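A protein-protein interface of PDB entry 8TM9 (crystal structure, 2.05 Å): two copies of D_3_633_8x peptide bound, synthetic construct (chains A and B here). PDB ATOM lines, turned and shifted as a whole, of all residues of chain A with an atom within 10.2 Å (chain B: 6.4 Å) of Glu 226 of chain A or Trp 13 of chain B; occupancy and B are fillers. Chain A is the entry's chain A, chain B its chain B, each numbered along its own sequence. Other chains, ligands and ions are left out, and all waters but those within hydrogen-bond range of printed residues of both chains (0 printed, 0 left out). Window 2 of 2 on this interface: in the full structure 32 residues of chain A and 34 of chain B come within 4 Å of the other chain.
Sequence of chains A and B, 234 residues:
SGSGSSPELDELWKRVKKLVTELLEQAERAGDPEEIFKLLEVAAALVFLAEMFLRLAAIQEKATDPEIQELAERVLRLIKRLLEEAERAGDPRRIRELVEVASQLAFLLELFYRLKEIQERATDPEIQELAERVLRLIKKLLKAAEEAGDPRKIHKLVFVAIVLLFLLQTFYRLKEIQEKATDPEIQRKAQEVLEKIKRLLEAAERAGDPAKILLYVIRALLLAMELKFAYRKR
CG1 of Val 47 of chain B touches CE2 of Phe 166 of chain A, 3.99 Å away.
Leu 221 of chain A touches Val 47 of chain B (CB to CG1, 3.8 Å).
O of Leu 222 of chain A touches CH2 of Trp 13 of chain B (3.9 Å).
Trp 13 of chain B touches Met 225 of chain A.
CG1 of Val 47 of chain B touches CE of Met 225 of chain A, 3.95 Å away.
CZ2 of Trp 13 of chain B touches CG of Glu 226 of chain A, at 3.4 Å.
Phe 229 of chain A touches Leu 9 of chain B.
Phe 229 of chain A touches Trp 13 of chain B (CE1 to CB, 3.6 Å).
Phe 229 of chain A touches Ala 50 of chain B (CZ to O, 3.2 Å).
Phe 229 of chain A touches Phe 53 of chain B.
Ala 220 of chain A touches none of the printed residues of chain B.
Of the printed residues of chain B, Leu 221 of chain A touches Val 47.
Of the printed residues of chain B, Met 225 of chain A touches Trp 13 (3.9 Å) and Val 47 (3.95 Å).
Glu 226 of chain A touches just one residue of chain B: Trp 13 (3.4 Å).
Lys 228 of chain A touches none of the printed residues of chain B.
No residue of chain A comes within 4 Å of Asp 10 of chain B.
No residue of chain A comes within 4 Å of Lys 14 of chain B.
No residue of chain A comes within 4 Å of Val 16 of chain B.
No residue of chain A comes within 4 Å of Lys 17 of chain B.
The nearest residue of chain A that does not touch Trp 13 of chain B is Leu 221 of chain A (6.0 Å).
The nearest printed residue of chain B that does not touch Phe 166 of chain A is Ala 50 of chain B (6.6 Å).
Hydrophobic or aromatic side chains of chain B that line the printed part of chain A: Trp 13, Val 47, Ala 50 and Phe 53.
Of the 25 printed residues of chain A, 6 touch a printed residue of chain B.
No position is printed for both chains.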
ATOM      1  N   PHE A 166     -31.017  29.414 -21.611  1.00  0.00           N
ATOM      2  CA  PHE A 166     -29.588  29.188 -21.797  1.00  0.00           C
ATOM      3  C   PHE A 166     -29.048  30.028 -22.948  1.00  0.00           C
ATOM      4  O   PHE A 166     -27.958  30.602 -22.850  1.00  0.00           O
ATOM      5  CB  PHE A 166     -29.330  27.698 -22.040  1.00  0.00           C
ATOM      6  CG  PHE A 166     -27.874  27.315 -22.035  1.00  0.00           C
ATOM      7  CD1 PHE A 166     -26.930  28.096 -21.386  1.00  0.00           C
ATOM      8  CD2 PHE A 166     -27.451  26.168 -22.685  1.00  0.00           C
ATOM      9  CE1 PHE A 166     -25.594  27.739 -21.388  1.00  0.00           C
ATOM     10  CE2 PHE A 166     -26.118  25.805 -22.690  1.00  0.00           C
ATOM     11  CZ  PHE A 166     -25.189  26.592 -22.040  1.00  0.00           C
ATOM     12  N   THR A 170     -26.096  33.039 -22.819  1.00  0.00           N
ATOM     13  CA  THR A 170     -24.898  33.108 -23.649  1.00  0.00           C
ATOM     14  C   THR A 170     -24.883  34.361 -24.514  1.00  0.00           C
ATOM     15  O   THR A 170     -23.807  34.847 -24.879  1.00  0.00           O
ATOM     16  CB  THR A 170     -24.783  31.860 -24.525  1.00  0.00           C
ATOM     17  OG1 THR A 170     -25.837  31.854 -25.496  1.00  0.00           O
ATOM     18  CG2 THR A 170     -24.864  30.599 -23.676  1.00  0.00           C
ATOM     19  N   ARG A 173     -23.131  36.909 -22.362  1.00  0.00           N
ATOM     20  CA  ARG A 173     -21.683  36.719 -22.345  1.00  0.00           C
ATOM     21  C   ARG A 173     -21.057  37.129 -23.672  1.00  0.00           C
ATOM     22  O   ARG A 173     -19.969  37.715 -23.698  1.00  0.00           O
ATOM     23  CB  ARG A 173     -21.354  35.262 -22.019  1.00  0.00           C
ATOM     24  CG  ARG A 173     -19.917  34.857 -22.317  1.00  0.00           C
ATOM     25  CD  ARG A 173     -19.055  34.895 -21.066  1.00  0.00           C
ATOM     26  NE  ARG A 173     -19.187  33.676 -20.278  1.00  0.00           N
ATOM     27  CZ  ARG A 173     -18.239  32.757 -20.154  1.00  0.00           C
ATOM     28  NH1 ARG A 173     -17.068  32.884 -20.756  1.00  0.00           N
ATOM     29  NH2 ARG A 173     -18.472  31.680 -19.407  1.00  0.00           N
ATOM     30  N   LEU A 174     -21.735  36.836 -24.785  1.00  0.00           N
ATOM     31  CA  LEU A 174     -21.198  37.203 -26.091  1.00  0.00           C
ATOM     32  C   LEU A 174     -21.111  38.716 -26.247  1.00  0.00           C
ATOM     33  O   LEU A 174     -20.155  39.233 -26.836  1.00  0.00           O
ATOM     34  CB  LEU A 174     -22.054  36.594 -27.201  1.00  0.00           C
ATOM     35  CG  LEU A 174     -21.438  35.396 -27.927  1.00  0.00           C
ATOM     36  CD1 LEU A 174     -20.150  35.800 -28.629  1.00  0.00           C
ATOM     37  CD2 LEU A 174     -21.185  34.254 -26.956  1.00  0.00           C
ATOM     38  N   ILE A 177     -18.171  39.645 -23.992  1.00  0.00           N
ATOM     39  CA  ILE A 177     -16.900  39.335 -24.642  1.00  0.00           C
ATOM     40  C   ILE A 177     -16.548  40.409 -25.661  1.00  0.00           C
ATOM     41  O   ILE A 177     -15.399  40.861 -25.740  1.00  0.00           O
ATOM     42  CB  ILE A 177     -16.963  37.938 -25.288  1.00  0.00           C
ATOM     43  CG1 ILE A 177     -16.794  36.847 -24.229  1.00  0.00           C
ATOM     44  CG2 ILE A 177     -15.909  37.797 -26.377  1.00  0.00           C
ATOM     45  CD1 ILE A 177     -16.967  35.443 -24.769  1.00  0.00           C
ATOM     46  N   ILE A 186     -12.027  40.279 -33.428  1.00  0.00           N
ATOM     47  CA  ILE A 186     -12.812  39.487 -32.489  1.00  0.00           C
ATOM     48  C   ILE A 186     -14.140  40.173 -32.195  1.00  0.00           C
ATOM     49  O   ILE A 186     -15.178  39.514 -32.063  1.00  0.00           O
ATOM     50  CB  ILE A 186     -11.997  39.226 -31.208  1.00  0.00           C
ATOM     51  CG1 ILE A 186     -10.994  38.095 -31.442  1.00  0.00           C
ATOM     52  CG2 ILE A 186     -12.904  38.873 -30.040  1.00  0.00           C
ATOM     53  N   LYS A 189     -16.199  39.365 -35.319  1.00  0.00           N
ATOM     54  CA  LYS A 189     -16.671  37.985 -35.341  1.00  0.00           C
ATOM     55  C   LYS A 189     -17.805  37.779 -34.343  1.00  0.00           C
ATOM     56  O   LYS A 189     -18.768  37.057 -34.625  1.00  0.00           O
ATOM     57  CB  LYS A 189     -15.515  37.028 -35.049  1.00  0.00           C
ATOM     58  CG  LYS A 189     -15.928  35.572 -34.913  1.00  0.00           C
ATOM     59  N   ALA A 190     -17.708  38.409 -33.170  1.00  0.00           N
ATOM     60  CA  ALA A 190     -18.804  38.350 -32.211  1.00  0.00           C
ATOM     61  C   ALA A 190     -20.049  39.031 -32.762  1.00  0.00           C
ATOM     62  O   ALA A 190     -21.163  38.517 -32.612  1.00  0.00           O
ATOM     63  CB  ALA A 190     -18.381  38.986 -30.887  1.00  0.00           C
ATOM     64  N   VAL A 193     -21.665  36.590 -35.128  1.00  0.00           N
ATOM     65  CA  VAL A 193     -22.357  35.531 -34.398  1.00  0.00           C
ATOM     66  C   VAL A 193     -23.600  36.078 -33.709  1.00  0.00           C
ATOM     67  O   VAL A 193     -24.646  35.417 -33.667  1.00  0.00           O
ATOM     68  CB  VAL A 193     -21.396  34.864 -33.393  1.00  0.00           C
ATOM     69  CG1 VAL A 193     -22.138  33.857 -32.527  1.00  0.00           C
ATOM     70  CG2 VAL A 193     -20.250  34.191 -34.129  1.00  0.00           C
ATOM     71  N   LYS A 196     -26.238  36.359 -36.301  1.00  0.00           N
ATOM     72  CA  LYS A 196     -26.747  35.049 -36.697  1.00  0.00           C
ATOM     73  C   LYS A 196     -27.703  34.490 -35.651  1.00  0.00           C
ATOM     74  O   LYS A 196     -28.693  33.834 -35.994  1.00  0.00           O
ATOM     75  CB  LYS A 196     -25.590  34.076 -36.936  1.00  0.00           C
ATOM     76  CG  LYS A 196     -24.793  34.339 -38.205  1.00  0.00           C
ATOM     77  CD  LYS A 196     -23.296  34.264 -37.952  1.00  0.00           C
ATOM     78  CE  LYS A 196     -22.825  32.833 -37.751  1.00  0.00           C
ATOM     79  NZ  LYS A 196     -22.355  32.224 -39.024  1.00  0.00           N
ATOM     80  N   ILE A 197     -27.421  34.734 -34.370  1.00  0.00           N
ATOM     81  CA  ILE A 197     -28.320  34.283 -33.312  1.00  0.00           C
ATOM     82  C   ILE A 197     -29.651  35.021 -33.395  1.00  0.00           C
ATOM     83  O   ILE A 197     -30.717  34.435 -33.173  1.00  0.00           O
ATOM     84  CB  ILE A 197     -27.652  34.456 -31.936  1.00  0.00           C
ATOM     85  CG1 ILE A 197     -26.455  33.512 -31.803  1.00  0.00           C
ATOM     86  CG2 ILE A 197     -28.649  34.209 -30.813  1.00  0.00           C
ATOM     87  CD1 ILE A 197     -25.620  33.756 -30.567  1.00  0.00           C
ATOM     88  N   ILE A 218     -30.785  25.373 -30.683  1.00  0.00           N
ATOM     89  CA  ILE A 218     -29.565  24.573 -30.606  1.00  0.00           C
ATOM     90  C   ILE A 218     -28.532  25.081 -31.603  1.00  0.00           C
ATOM     91  O   ILE A 218     -27.339  25.185 -31.287  1.00  0.00           O
ATOM     92  CB  ILE A 218     -29.887  23.084 -30.831  1.00  0.00           C
ATOM     93  CG1 ILE A 218     -30.588  22.499 -29.606  1.00  0.00           C
ATOM     94  CG2 ILE A 218     -28.623  22.297 -31.145  1.00  0.00           C
ATOM     95  CD1 ILE A 218     -31.204  21.146 -29.855  1.00  0.00           C
ATOM     96  N   ARG A 219     -28.972  25.415 -32.819  1.00  0.00           N
ATOM     97  CA  ARG A 219     -28.055  25.953 -33.818  1.00  0.00           C
ATOM     98  C   ARG A 219     -27.472  27.286 -33.368  1.00  0.00           C
ATOM     99  O   ARG A 219     -26.292  27.569 -33.607  1.00  0.00           O
ATOM    100  CB  ARG A 219     -28.772  26.106 -35.159  1.00  0.00           C
ATOM    101  CG  ARG A 219     -29.088  24.790 -35.853  1.00  0.00           C
ATOM    102  CD  ARG A 219     -30.018  25.001 -37.039  1.00  0.00           C
ATOM    103  NE  ARG A 219     -29.461  25.937 -38.009  1.00  0.00           N
ATOM    104  CZ  ARG A 219     -30.084  26.335 -39.110  1.00  0.00           C
ATOM    105  NH1 ARG A 219     -31.295  25.899 -39.415  1.00  0.00           N
ATOM    106  NH2 ARG A 219     -29.477  27.192 -39.926  1.00  0.00           N
ATOM    107  N   ALA A 220     -28.283  28.120 -32.713  1.00  0.00           N
ATOM    108  CA  ALA A 220     -27.779  29.390 -32.204  1.00  0.00           C
ATOM    109  C   ALA A 220     -26.833  29.187 -31.029  1.00  0.00           C
ATOM    110  O   ALA A 220     -25.868  29.944 -30.874  1.00  0.00           O
ATOM    111  CB  ALA A 220     -28.942  30.296 -31.802  1.00  0.00           C
ATOM    112  N   LEU A 221     -27.091  28.179 -30.192  1.00  0.00           N
ATOM    113  CA  LEU A 221     -26.185  27.889 -29.087  1.00  0.00           C
ATOM    114  C   LEU A 221     -24.864  27.318 -29.582  1.00  0.00           C
ATOM    115  O   LEU A 221     -23.842  27.441 -28.898  1.00  0.00           O
ATOM    116  CB  LEU A 221     -26.845  26.923 -28.104  1.00  0.00           C
ATOM    117  CG  LEU A 221     -27.581  27.553 -26.921  1.00  0.00           C
ATOM    118  CD1 LEU A 221     -28.370  26.499 -26.165  1.00  0.00           C
ATOM    119  CD2 LEU A 221     -26.602  28.257 -25.995  1.00  0.00           C
ATOM    120  N   LEU A 222     -24.864  26.692 -30.761  1.00  0.00           N
ATOM    121  CA  LEU A 222     -23.625  26.167 -31.322  1.00  0.00           C
ATOM    122  C   LEU A 222     -22.670  27.295 -31.690  1.00  0.00           C
ATOM    123  O   LEU A 222     -21.478  27.244 -31.366  1.00  0.00           O
ATOM    124  CB  LEU A 222     -23.930  25.298 -32.543  1.00  0.00           C
ATOM    125  CG  LEU A 222     -23.086  24.035 -32.722  1.00  0.00           C
ATOM    126  CD1 LEU A 222     -22.916  23.302 -31.399  1.00  0.00           C
ATOM    127  CD2 LEU A 222     -23.704  23.124 -33.773  1.00  0.00           C
ATOM    128  N   LEU A 223     -23.180  28.328 -32.367  1.00  0.00           N
ATOM    129  CA  LEU A 223     -22.329  29.449 -32.757  1.00  0.00           C
ATOM    130  C   LEU A 223     -21.863  30.241 -31.542  1.00  0.00           C
ATOM    131  O   LEU A 223     -20.717  30.704 -31.499  1.00  0.00           O
ATOM    132  CB  LEU A 223     -23.075  30.359 -33.732  1.00  0.00           C
ATOM    133  CG  LEU A 223     -23.927  29.674 -34.803  1.00  0.00           C
ATOM    134  CD1 LEU A 223     -25.082  30.571 -35.220  1.00  0.00           C
ATOM    135  CD2 LEU A 223     -23.075  29.298 -36.005  1.00  0.00           C
ATOM    136  N   ALA A 224     -22.737  30.410 -30.547  1.00  0.00           N
ATOM    137  CA  ALA A 224     -22.359  31.153 -29.349  1.00  0.00           C
ATOM    138  C   ALA A 224     -21.293  30.422 -28.545  1.00  0.00           C
ATOM    139  O   ALA A 224     -20.429  31.063 -27.936  1.00  0.00           O
ATOM    140  CB  ALA A 224     -23.589  31.419 -28.483  1.00  0.00           C
ATOM    141  N   MET A 225     -21.335  29.087 -28.529  1.00  0.00           N
ATOM    142  CA  MET A 225     -20.332  28.324 -27.797  1.00  0.00           C
ATOM    143  C   MET A 225     -18.990  28.292 -28.520  1.00  0.00           C
ATOM    144  O   MET A 225     -17.962  28.057 -27.876  1.00  0.00           O
ATOM    145  CB  MET A 225     -20.834  26.900 -27.550  1.00  0.00           C
ATOM    146  CG  MET A 225     -20.129  26.179 -26.407  1.00  0.00           C
ATOM    147  SD  MET A 225     -20.380  26.968 -24.804  1.00  0.00           S
ATOM    148  CE  MET A 225     -22.162  27.139 -24.774  1.00  0.00           C
ATOM    149  N   GLU A 226     -18.976  28.523 -29.835  1.00  0.00           N
ATOM    150  CA  GLU A 226     -17.711  28.611 -30.558  1.00  0.00           C
ATOM    151  C   GLU A 226     -16.882  29.789 -30.063  1.00  0.00           C
ATOM    152  O   GLU A 226     -15.701  29.638 -29.726  1.00  0.00           O
ATOM    153  CB  GLU A 226     -17.966  28.733 -32.061  1.00  0.00           C
ATOM    154  CG  GLU A 226     -18.647  27.531 -32.690  1.00  0.00           C
ATOM    155  N   LEU A 227     -17.488  30.977 -30.012  1.00  0.00           N
ATOM    156  CA  LEU A 227     -16.767  32.159 -29.554  1.00  0.00           C
ATOM    157  C   LEU A 227     -16.481  32.101 -28.060  1.00  0.00           C
ATOM    158  O   LEU A 227     -15.488  32.674 -27.599  1.00  0.00           O
ATOM    159  CB  LEU A 227     -17.558  33.421 -29.894  1.00  0.00           C
ATOM    160  CG  LEU A 227     -17.824  33.662 -31.381  1.00  0.00           C
ATOM    161  N   LYS A 228     -17.335  31.421 -27.289  1.00  0.00           N
ATOM    162  CA  LYS A 228     -17.082  31.282 -25.859  1.00  0.00           C
ATOM    163  C   LYS A 228     -15.840  30.443 -25.590  1.00  0.00           C
ATOM    164  O   LYS A 228     -15.151  30.661 -24.587  1.00  0.00           O
ATOM    165  CB  LYS A 228     -18.299  30.671 -25.165  1.00  0.00           C
ATOM    166  N   PHE A 229     -15.538  29.487 -26.471  1.00  0.00           N
ATOM    167  CA  PHE A 229     -14.332  28.682 -26.314  1.00  0.00           C
ATOM    168  C   PHE A 229     -13.113  29.383 -26.903  1.00  0.00           C
ATOM    169  O   PHE A 229     -12.013  29.295 -26.346  1.00  0.00           O
ATOM    170  CB  PHE A 229     -14.525  27.312 -26.964  1.00  0.00           C
ATOM    171  CG  PHE A 229     -15.072  26.271 -26.030  1.00  0.00           C
ATOM    172  CD1 PHE A 229     -14.220  25.479 -25.279  1.00  0.00           C
ATOM    173  CD2 PHE A 229     -16.438  26.087 -25.899  1.00  0.00           C
ATOM    174  CE1 PHE A 229     -14.720  24.521 -24.417  1.00  0.00           C
ATOM    175  CE2 PHE A 229     -16.944  25.131 -25.039  1.00  0.00           C
ATOM    176  CZ  PHE A 229     -16.084  24.347 -24.296  1.00  0.00           C
ATOM    177  N   ALA A 230     -13.289  30.084 -28.026  1.00  0.00           N
ATOM    178  CA  ALA A 230     -12.198  30.817 -28.666  1.00  0.00           C
ATOM    179  C   ALA A 230     -12.065  32.193 -28.010  1.00  0.00           C
ATOM    180  O   ALA A 230     -12.291  33.243 -28.615  1.00  0.00           O
ATOM    181  CB  ALA A 230     -12.433  30.927 -30.165  1.00  0.00           C
ATOM    182  N   TYR A 231     -11.691  32.167 -26.734  1.00  0.00           N
ATOM    183  CA  TYR A 231     -11.509  33.389 -25.959  1.00  0.00           C
ATOM    184  C   TYR A 231     -10.652  33.126 -24.725  1.00  0.00           C
ATOM    185  O   TYR A 231     -10.534  31.988 -24.271  1.00  0.00           O
ATOM    186  CB  TYR A 231     -12.861  33.973 -25.547  1.00  0.00           C
ATOM    187  CG  TYR A 231     -12.775  35.372 -24.980  1.00  0.00           C
ATOM    188  CD1 TYR A 231     -12.557  36.465 -25.809  1.00  0.00           C
ATOM    189  CD2 TYR A 231     -12.911  35.601 -23.617  1.00  0.00           C
ATOM    190  CE1 TYR A 231     -12.476  37.746 -25.296  1.00  0.00           C
ATOM    191  CE2 TYR A 231     -12.833  36.878 -23.095  1.00  0.00           C
ATOM    192  CZ  TYR A 231     -12.615  37.947 -23.939  1.00  0.00           C
ATOM    193  OH  TYR A 231     -12.536  39.220 -23.424  1.00  0.00           O
ATOM    194  N   GLU B   8      -6.439  21.058 -23.099  1.00  0.00           N
ATOM    195  CA  GLU B   8      -7.153  19.940 -23.702  1.00  0.00           C
ATOM    196  C   GLU B   8      -8.635  20.224 -23.912  1.00  0.00           C
ATOM    197  O   GLU B   8      -9.337  19.377 -24.474  1.00  0.00           O
ATOM    198  CB  GLU B   8      -6.985  18.683 -22.843  1.00  0.00           C
ATOM    199  CG  GLU B   8      -7.739  18.717 -21.525  1.00  0.00           C
ATOM    200  CD  GLU B   8      -7.361  17.569 -20.610  1.00  0.00           C
ATOM    201  OE1 GLU B   8      -6.341  17.684 -19.898  1.00  0.00           O
ATOM    202  OE2 GLU B   8      -8.083  16.549 -20.603  1.00  0.00           O
ATOM    203  N   LEU B   9      -9.127  21.387 -23.477  1.00  0.00           N
ATOM    204  CA  LEU B   9     -10.524  21.736 -23.702  1.00  0.00           C
ATOM    205  C   LEU B   9     -10.796  22.123 -25.150  1.00  0.00           C
ATOM    206  O   LEU B   9     -11.948  22.045 -25.591  1.00  0.00           O
ATOM    207  CB  LEU B   9     -10.939  22.875 -22.770  1.00  0.00           C
ATOM    208  N   ASP B  10      -9.768  22.539 -25.892  1.00  0.00           N
ATOM    209  CA  ASP B  10      -9.964  22.891 -27.296  1.00  0.00           C
ATOM    210  C   ASP B  10     -10.349  21.677 -28.130  1.00  0.00           C
ATOM    211  O   ASP B  10     -11.130  21.802 -29.080  1.00  0.00           O
ATOM    212  CB  ASP B  10      -8.699  23.541 -27.855  1.00  0.00           C
ATOM    213  N   GLU B  11      -9.815  20.502 -27.796  1.00  0.00           N
ATOM    214  CA  GLU B  11     -10.167  19.277 -28.504  1.00  0.00           C
ATOM    215  C   GLU B  11     -11.413  18.612 -27.938  1.00  0.00           C
ATOM    216  O   GLU B  11     -12.144  17.950 -28.684  1.00  0.00           O
ATOM    217  CB  GLU B  11      -8.998  18.288 -28.473  1.00  0.00           C
ATOM    218  CG  GLU B  11      -7.634  18.916 -28.729  1.00  0.00           C
ATOM    219  CD  GLU B  11      -6.987  19.452 -27.467  1.00  0.00           C
ATOM    220  OE1 GLU B  11      -6.930  20.690 -27.310  1.00  0.00           O
ATOM    221  OE2 GLU B  11      -6.536  18.638 -26.634  1.00  0.00           O
ATOM    222  N   LEU B  12     -11.669  18.766 -26.637  1.00  0.00           N
ATOM    223  CA  LEU B  12     -12.911  18.254 -26.068  1.00  0.00           C
ATOM    224  C   LEU B  12     -14.117  18.955 -26.678  1.00  0.00           C
ATOM    225  O   LEU B  12     -15.133  18.316 -26.975  1.00  0.00           O
ATOM    226  CB  LEU B  12     -12.903  18.419 -24.549  1.00  0.00           C
ATOM    227  CG  LEU B  12     -12.323  17.254 -23.744  1.00  0.00           C
ATOM    228  N   TRP B  13     -14.021  20.273 -26.875  1.00  0.00           N
ATOM    229  CA  TRP B  13     -15.091  20.994 -27.552  1.00  0.00           C
ATOM    230  C   TRP B  13     -15.200  20.582 -29.015  1.00  0.00           C
ATOM    231  O   TRP B  13     -16.308  20.538 -29.564  1.00  0.00           O
ATOM    232  CB  TRP B  13     -14.863  22.502 -27.440  1.00  0.00           C
ATOM    233  CG  TRP B  13     -15.265  23.255 -28.668  1.00  0.00           C
ATOM    234  CD1 TRP B  13     -14.435  23.780 -29.616  1.00  0.00           C
ATOM    235  CD2 TRP B  13     -16.599  23.560 -29.088  1.00  0.00           C
ATOM    236  NE1 TRP B  13     -15.171  24.395 -30.599  1.00  0.00           N
ATOM    237  CE2 TRP B  13     -16.502  24.273 -30.298  1.00  0.00           C
ATOM    238  CE3 TRP B  13     -17.866  23.298 -28.558  1.00  0.00           C
ATOM    239  CZ2 TRP B  13     -17.623  24.730 -30.987  1.00  0.00           C
ATOM    240  CZ3 TRP B  13     -18.978  23.753 -29.243  1.00  0.00           C
ATOM    241  CH2 TRP B  13     -18.849  24.461 -30.444  1.00  0.00           C
ATOM    242  N   LYS B  14     -14.071  20.276 -29.659  1.00  0.00           N
ATOM    243  CA  LYS B  14     -14.110  19.806 -31.039  1.00  0.00           C
ATOM    244  C   LYS B  14     -14.874  18.492 -31.148  1.00  0.00           C
ATOM    245  O   LYS B  14     -15.592  18.260 -32.128  1.00  0.00           O
ATOM    246  CB  LYS B  14     -12.690  19.651 -31.584  1.00  0.00           C
ATOM    247  N   ARG B  15     -14.731  17.619 -30.148  1.00  0.00           N
ATOM    248  CA  ARG B  15     -15.516  16.389 -30.127  1.00  0.00           C
ATOM    249  C   ARG B  15     -16.986  16.682 -29.859  1.00  0.00           C
ATOM    250  O   ARG B  15     -17.869  16.019 -30.416  1.00  0.00           O
ATOM    251  CB  ARG B  15     -14.964  15.430 -29.073  1.00  0.00           C
ATOM    252  CG  ARG B  15     -13.543  14.962 -29.331  1.00  0.00           C
ATOM    253  CD  ARG B  15     -13.113  13.937 -28.294  1.00  0.00           C
ATOM    254  NE  ARG B  15     -11.782  13.406 -28.564  1.00  0.00           N
ATOM    255  CZ  ARG B  15     -11.533  12.404 -29.396  1.00  0.00           C
ATOM    256  NH1 ARG B  15     -12.503  11.797 -30.059  1.00  0.00           N
ATOM    257  NH2 ARG B  15     -10.277  12.000 -29.566  1.00  0.00           N
ATOM    258  N   VAL B  16     -17.266  17.671 -29.008  1.00  0.00           N
ATOM    259  CA  VAL B  16     -18.647  18.007 -28.679  1.00  0.00           C
ATOM    260  C   VAL B  16     -19.359  18.587 -29.895  1.00  0.00           C
ATOM    261  O   VAL B  16     -20.474  18.176 -30.237  1.00  0.00           O
ATOM    262  CB  VAL B  16     -18.692  18.975 -27.482  1.00  0.00           C
ATOM    263  CG1 VAL B  16     -20.006  19.744 -27.462  1.00  0.00           C
ATOM    264  CG2 VAL B  16     -18.493  18.216 -26.178  1.00  0.00           C
ATOM    265  N   LYS B  17     -18.721  19.546 -30.572  1.00  0.00           N
ATOM    266  CA  LYS B  17     -19.357  20.185 -31.720  1.00  0.00           C
ATOM    267  C   LYS B  17     -19.571  19.202 -32.864  1.00  0.00           C
ATOM    268  O   LYS B  17     -20.509  19.366 -33.651  1.00  0.00           O
ATOM    269  CB  LYS B  17     -18.526  21.383 -32.184  1.00  0.00           C
ATOM    270  CG  LYS B  17     -17.268  21.026 -32.960  1.00  0.00           C
ATOM    271  N   LYS B  18     -18.727  18.173 -32.967  1.00  0.00           N
ATOM    272  CA  LYS B  18     -18.913  17.175 -34.014  1.00  0.00           C
ATOM    273  C   LYS B  18     -20.123  16.296 -33.726  1.00  0.00           C
ATOM    274  O   LYS B  18     -20.882  15.954 -34.640  1.00  0.00           O
ATOM    275  CB  LYS B  18     -17.652  16.324 -34.157  1.00  0.00           C
ATOM    276  CG  LYS B  18     -17.713  15.301 -35.280  1.00  0.00           C
ATOM    277  N   VAL B  47     -24.286  20.695 -25.737  1.00  0.00           N
ATOM    278  CA  VAL B  47     -23.920  22.105 -25.660  1.00  0.00           C
ATOM    279  C   VAL B  47     -23.790  22.538 -24.205  1.00  0.00           C
ATOM    280  O   VAL B  47     -22.826  23.213 -23.824  1.00  0.00           O
ATOM    281  CB  VAL B  47     -24.944  22.967 -26.421  1.00  0.00           C
ATOM    282  CG1 VAL B  47     -24.695  24.445 -26.165  1.00  0.00           C
ATOM    283  CG2 VAL B  47     -24.891  22.660 -27.911  1.00  0.00           C
ATOM    284  N   ALA B  50     -20.563  21.367 -22.844  1.00  0.00           N
ATOM    285  CA  ALA B  50     -19.422  22.218 -23.163  1.00  0.00           C
ATOM    286  C   ALA B  50     -19.365  23.447 -22.266  1.00  0.00           C
ATOM    287  O   ALA B  50     -18.279  23.985 -22.023  1.00  0.00           O
ATOM    288  CB  ALA B  50     -19.471  22.634 -24.632  1.00  0.00           C
ATOM    289  N   PHE B  53     -17.387  22.852 -19.144  1.00  0.00           N
ATOM    290  CA  PHE B  53     -15.938  22.852 -19.313  1.00  0.00           C
ATOM    291  C   PHE B  53     -15.321  24.175 -18.879  1.00  0.00           C
ATOM    292  O   PHE B  53     -14.152  24.211 -18.478  1.00  0.00           O
ATOM    293  CB  PHE B  53     -15.576  22.561 -20.770  1.00  0.00           C
ATOM    294  CG  PHE B  53     -15.879  21.155 -21.206  1.00  0.00           C
ATOM    295  CD1 PHE B  53     -16.041  20.144 -20.274  1.00  0.00           C
ATOM    296  CD2 PHE B  53     -16.001  20.847 -22.551  1.00  0.00           C
ATOM    297  CE1 PHE B  53     -16.319  18.850 -20.677  1.00  0.00           C
ATOM    298  CE2 PHE B  53     -16.279  19.557 -22.960  1.00  0.00           C
ATOM    299  CZ  PHE B  53     -16.438  18.557 -22.022  1.00  0.00           C
